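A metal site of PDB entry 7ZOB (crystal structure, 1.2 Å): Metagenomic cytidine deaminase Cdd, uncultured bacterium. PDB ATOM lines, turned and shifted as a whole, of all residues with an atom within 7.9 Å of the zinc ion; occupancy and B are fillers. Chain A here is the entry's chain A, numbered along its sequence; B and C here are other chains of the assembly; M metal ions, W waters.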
ATOM      1  N   VAL A  26      15.771 -18.076  19.268  1.00  0.00           N
ATOM      2  CA  VAL A  26      16.290 -17.150  18.273  1.00  0.00           C
ATOM      3  C   VAL A  26      17.170 -16.134  18.991  1.00  0.00           C
ATOM      4  O   VAL A  26      16.775 -15.608  20.030  1.00  0.00           O
ATOM      5  CB  VAL A  26      15.146 -16.398  17.566  1.00  0.00           C
ATOM      6  CG1 VAL A  26      15.709 -15.431  16.520  1.00  0.00           C
ATOM      7  CG2 VAL A  26      14.183 -17.343  16.926  1.00  0.00           C
ATOM      8  N   ASN A  42      14.133 -14.113  21.614  1.00  0.00           N
ATOM      9  CA  ASN A  42      12.680 -14.271  21.653  1.00  0.00           C
ATOM     10  C   ASN A  42      12.190 -14.512  23.070  1.00  0.00           C
ATOM     11  O   ASN A  42      12.850 -15.181  23.876  1.00  0.00           O
ATOM     12  CB  ASN A  42      12.162 -15.316  20.668  1.00  0.00           C
ATOM     13  CG  ASN A  42      12.742 -16.697  20.892  1.00  0.00           C
ATOM     14  OD1 ASN A  42      13.975 -16.853  21.069  1.00  0.00           O
ATOM     15  ND2 ASN A  42      11.895 -17.710  20.822  1.00  0.00           N
ATOM     16  N   THR A  51       3.947 -12.785  22.549  1.00  0.00           N
ATOM     17  CA  THR A  51       5.334 -13.161  22.299  1.00  0.00           C
ATOM     18  C   THR A  51       6.072 -12.086  21.517  1.00  0.00           C
ATOM     19  O   THR A  51       5.509 -11.480  20.594  1.00  0.00           O
ATOM     20  CB  THR A  51       5.330 -14.473  21.496  1.00  0.00           C
ATOM     21  OG1 THR A  51       4.787 -15.491  22.337  1.00  0.00           O
ATOM     22  CG2 THR A  51       6.705 -14.859  21.013  1.00  0.00           C
ATOM     23  N   ASN A  52       7.344 -11.867  21.853  1.00  0.00           N
ATOM     24  CA  ASN A  52       8.201 -10.974  21.084  1.00  0.00           C
ATOM     25  C   ASN A  52       9.337 -11.740  20.443  1.00  0.00           C
ATOM     26  O   ASN A  52       9.906 -12.669  21.036  1.00  0.00           O
ATOM     27  CB  ASN A  52       8.775  -9.872  21.978  1.00  0.00           C
ATOM     28  CG  ASN A  52       9.378  -8.712  21.173  1.00  0.00           C
ATOM     29  OD1 ASN A  52      10.550  -8.354  21.344  1.00  0.00           O
ATOM     30  ND2 ASN A  52       8.603  -8.131  20.270  1.00  0.00           N
ATOM     31  N   CYS A  53       9.692 -11.332  19.247  1.00  0.00           N
ATOM     32  CA  CYS A  53      10.790 -11.944  18.522  1.00  0.00           C
ATOM     33  C   CYS A  53      12.133 -11.361  18.921  1.00  0.00           C
ATOM     34  O   CYS A  53      12.232 -10.199  19.341  1.00  0.00           O
ATOM     35  CB  CYS A  53      10.587 -11.712  17.012  1.00  0.00           C
ATOM     36  SG  CYS A  53       9.146 -12.597  16.334  1.00  0.00           S
ATOM     37  N   GLY A  54      13.183 -12.156  18.749  1.00  0.00           N
ATOM     38  CA  GLY A  54      14.511 -11.699  19.154  1.00  0.00           C
ATOM     39  C   GLY A  54      15.024 -10.481  18.425  1.00  0.00           C
ATOM     40  O   GLY A  54      15.640  -9.595  19.029  1.00  0.00           O
ATOM     41  N   GLU A  55      14.786 -10.406  17.122  1.00  0.00           N
ATOM     42  CA  GLU A  55      15.289  -9.263  16.385  1.00  0.00           C
ATOM     43  C   GLU A  55      14.548  -7.992  16.780  1.00  0.00           C
ATOM     44  O   GLU A  55      15.155  -6.900  16.792  1.00  0.00           O
ATOM     45  CB  GLU A  55      15.313  -9.536  14.877  1.00  0.00           C
ATOM     46  CG  GLU A  55      14.000  -9.910  14.275  1.00  0.00           C
ATOM     47  CD  GLU A  55      13.645 -11.431  14.322  1.00  0.00           C
ATOM     48  OE1 GLU A  55      13.687 -12.066  15.393  1.00  0.00           O
ATOM     49  OE2 GLU A  55      13.262 -11.970  13.264  1.00  0.00           O
ATOM     50  N   ARG A  56      13.277  -8.100  17.156  1.00  0.00           N
ATOM     51  CA  ARG A  56      12.576  -6.939  17.710  1.00  0.00           C
ATOM     52  C   ARG A  56      13.151  -6.561  19.075  1.00  0.00           C
ATOM     53  O   ARG A  56      13.346  -5.384  19.360  1.00  0.00           O
ATOM     54  CB  ARG A  56      11.069  -7.194  17.778  1.00  0.00           C
ATOM     55  CG  ARG A  56      10.400  -6.973  16.406  1.00  0.00           C
ATOM     56  CD  ARG A  56       8.885  -7.074  16.479  1.00  0.00           C
ATOM     57  NE  ARG A  56       8.456  -8.467  16.571  1.00  0.00           N
ATOM     58  CZ  ARG A  56       7.325  -8.877  17.144  1.00  0.00           C
ATOM     59  NH1 ARG A  56       6.459  -8.019  17.665  1.00  0.00           N
ATOM     60  NH2 ARG A  56       7.067 -10.192  17.205  1.00  0.00           N
ATOM     61  N   ILE A  77      20.815 -12.225  12.937  1.00  0.00           N
ATOM     62  CA  ILE A  77      19.701 -12.998  13.474  1.00  0.00           C
ATOM     63  C   ILE A  77      20.021 -14.471  13.253  1.00  0.00           C
ATOM     64  O   ILE A  77      20.314 -14.869  12.114  1.00  0.00           O
ATOM     65  CB  ILE A  77      18.357 -12.658  12.805  1.00  0.00           C
ATOM     66  CG1 ILE A  77      18.115 -11.157  12.739  1.00  0.00           C
ATOM     67  CG2 ILE A  77      17.214 -13.349  13.552  1.00  0.00           C
ATOM     68  CD1 ILE A  77      16.944 -10.795  11.826  1.00  0.00           C
ATOM     69  N   ALA A  86      14.629 -16.418   7.989  1.00  0.00           N
ATOM     70  CA  ALA A  86      14.526 -14.983   7.870  1.00  0.00           C
ATOM     71  C   ALA A  86      13.606 -14.451   8.965  1.00  0.00           C
ATOM     72  O   ALA A  86      12.791 -15.193   9.542  1.00  0.00           O
ATOM     73  CB  ALA A  86      13.948 -14.632   6.493  1.00  0.00           C
ATOM     74  N   PRO A  87      13.683 -13.157   9.276  1.00  0.00           N
ATOM     75  CA  PRO A  87      12.706 -12.570  10.209  1.00  0.00           C
ATOM     76  C   PRO A  87      11.280 -12.812   9.721  1.00  0.00           C
ATOM     77  O   PRO A  87      11.030 -12.837   8.509  1.00  0.00           O
ATOM     78  CB  PRO A  87      13.060 -11.073  10.207  1.00  0.00           C
ATOM     79  CG  PRO A  87      13.913 -10.861   8.950  1.00  0.00           C
ATOM     80  CD  PRO A  87      14.606 -12.156   8.711  1.00  0.00           C
ATOM     81  N   CYS A  88      10.378 -13.014  10.660  1.00  0.00           N
ATOM     82  CA  CYS A  88       8.968 -13.212  10.295  1.00  0.00           C
ATOM     83  C   CYS A  88       8.370 -11.894   9.774  1.00  0.00           C
ATOM     84  O   CYS A  88       8.998 -10.835   9.810  1.00  0.00           O
ATOM     85  CB  CYS A  88       8.163 -13.701  11.499  1.00  0.00           C
ATOM     86  SG  CYS A  88       7.688 -12.439  12.710  1.00  0.00           S
ATOM     87  N   GLY A  89       7.148 -11.979   9.262  1.00  0.00           N
ATOM     88  CA  GLY A  89       6.536 -10.800   8.671  1.00  0.00           C
ATOM     89  C   GLY A  89       6.342  -9.659   9.654  1.00  0.00           C
ATOM     90  O   GLY A  89       6.439  -8.491   9.264  1.00  0.00           O
ATOM     91  N   ILE A  90       6.047  -9.960  10.932  1.00  0.00           N
ATOM     92  CA  ILE A  90       5.942  -8.883  11.927  1.00  0.00           C
ATOM     93  C   ILE A  90       7.263  -8.113  11.995  1.00  0.00           C
ATOM     94  O   ILE A  90       7.314  -6.866  11.938  1.00  0.00           O
ATOM     95  CB  ILE A  90       5.584  -9.423  13.319  1.00  0.00           C
ATOM     96  CG1 ILE A  90       4.327 -10.275  13.309  1.00  0.00           C
ATOM     97  CG2 ILE A  90       5.488  -8.242  14.309  1.00  0.00           C
ATOM     98  CD1 ILE A  90       4.196 -11.065  14.625  1.00  0.00           C
ATOM     99  N   CYS A  91       8.363  -8.866  12.135  1.00  0.00           N
ATOM    100  CA  CYS A  91       9.669  -8.274  12.267  1.00  0.00           C
ATOM    101  C   CYS A  91      10.068  -7.539  11.007  1.00  0.00           C
ATOM    102  O   CYS A  91      10.702  -6.472  11.077  1.00  0.00           O
ATOM    103  CB  CYS A  91      10.677  -9.377  12.575  1.00  0.00           C
ATOM    104  SG  CYS A  91      10.444  -9.977  14.267  1.00  0.00           S
ATOM    105  N   ARG A  92       9.669  -8.025   9.848  1.00  0.00           N
ATOM    106  CA  ARG A  92       9.961  -7.295   8.608  1.00  0.00           C
ATOM    107  C   ARG A  92       9.264  -5.944   8.577  1.00  0.00           C
ATOM    108  O   ARG A  92       9.836  -4.968   8.125  1.00  0.00           O
ATOM    109  CB  ARG A  92       9.586  -8.119   7.381  1.00  0.00           C
ATOM    110  CG  ARG A  92      10.441  -9.359   7.230  1.00  0.00           C
ATOM    111  CD  ARG A  92      10.060 -10.172   6.011  1.00  0.00           C
ATOM    112  NE  ARG A  92      10.381 -11.584   6.211  1.00  0.00           N
ATOM    113  CZ  ARG A  92      10.384 -12.498   5.255  1.00  0.00           C
ATOM    114  NH1 ARG A  92      10.148 -12.147   3.994  1.00  0.00           N
ATOM    115  NH2 ARG A  92      10.658 -13.757   5.554  1.00  0.00           N
ATOM    116  N   SER B  47       4.667 -18.042  13.761  1.00  0.00           N
ATOM    117  CA  SER B  47       5.240 -16.922  14.512  1.00  0.00           C
ATOM    118  C   SER B  47       4.240 -16.578  15.621  1.00  0.00           C
ATOM    119  O   SER B  47       3.187 -15.972  15.350  1.00  0.00           O
ATOM    120  CB  SER B  47       5.475 -15.737  13.588  1.00  0.00           C
ATOM    121  OG  SER B  47       6.166 -14.740  14.345  1.00  0.00           O
ATOM    122  N   TYR B  48       4.536 -16.993  16.859  1.00  0.00           N
ATOM    123  CA  TYR B  48       3.494 -17.001  17.884  1.00  0.00           C
ATOM    124  C   TYR B  48       2.877 -15.633  18.106  1.00  0.00           C
ATOM    125  O   TYR B  48       1.674 -15.535  18.406  1.00  0.00           O
ATOM    126  CB  TYR B  48       4.033 -17.521  19.215  1.00  0.00           C
ATOM    127  CG  TYR B  48       4.181 -19.031  19.328  1.00  0.00           C
ATOM    128  CD1 TYR B  48       3.937 -19.886  18.260  1.00  0.00           C
ATOM    129  CD2 TYR B  48       4.569 -19.580  20.531  1.00  0.00           C
ATOM    130  CE1 TYR B  48       4.110 -21.264  18.393  1.00  0.00           C
ATOM    131  CE2 TYR B  48       4.701 -20.953  20.679  1.00  0.00           C
ATOM    132  CZ  TYR B  48       4.498 -21.781  19.604  1.00  0.00           C
ATOM    133  OH  TYR B  48       4.658 -23.161  19.743  1.00  0.00           O
ATOM    134  N   GLY B  49       3.665 -14.555  17.957  1.00  0.00           N
ATOM    135  CA  GLY B  49       3.155 -13.218  18.184  1.00  0.00           C
ATOM    136  C   GLY B  49       2.068 -12.789  17.214  1.00  0.00           C
ATOM    137  O   GLY B  49       1.385 -11.807  17.485  1.00  0.00           O
ATOM    138  N   GLN C  93       2.445 -12.430   7.390  1.00  0.00           N
ATOM    139  CA  GLN C  93       2.784 -13.590   8.199  1.00  0.00           C
ATOM    140  C   GLN C  93       1.534 -14.449   8.445  1.00  0.00           C
ATOM    141  O   GLN C  93       1.595 -15.685   8.385  1.00  0.00           O
ATOM    142  CB  GLN C  93       3.422 -13.144   9.531  1.00  0.00           C
ATOM    143  CG  GLN C  93       3.889 -14.283  10.394  1.00  0.00           C
ATOM    144  CD  GLN C  93       4.932 -15.131   9.731  1.00  0.00           C
ATOM    145  OE1 GLN C  93       5.865 -14.592   9.103  1.00  0.00           O
ATOM    146  NE2 GLN C  93       4.813 -16.450   9.863  1.00  0.00           N
HETATM  147 ZN    ZN M   1       9.498 -12.071  14.131  1.00  0.00          ZN
HETATM  148  O   HOH W   1      10.995 -13.207  13.407  1.00  0.00           O
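The side-chain sulfur (SG) of Cys 53 sits close to the guanidinium group (NH2) of Arg 56 (3.3 Å).
The side-chain sulfur (SG) of Cys 91 lies close to the side-chain carboxylate (OE2) of Glu 55 (3.6 Å).
The guanidinium group of Arg 56 lies close to the side-chain sulfur of Cys 91, 3.4 Å away.
The side-chain hydroxyl of Ser 47 of chain B lies close to the side-chain sulfur of Cys 88, at 3.2 Å.
The side-chain sulfur of Cys 88 lies close to the backbone NH of Ile 90.
The zinc ion is bound by water W1, at 2.0 Å.
The side-chain sulfur (SG) of Cys 53 binds the zinc ion (2.3 Å).
SG of Cys 91 binds the zinc ion (2.3 Å).
SG of Cys 88 binds the zinc ion, 2.3 Å away.
The zinc ion has four donor atoms within binding distance.
Water W1 bridges OE2 of Glu 55 (2.6 Å) and N of Cys 88 (2.8 Å).
Residues that only touch the zinc ion: Glu 55 (3.9 Å).
Four residues have an atom within 4 Å of the zinc ion: Cys 53, Glu 55, Cys 88 and Cys 91.
The nearest printed residue that does not touch the zinc ion is Ser 47 of chain B (4.3 Å).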
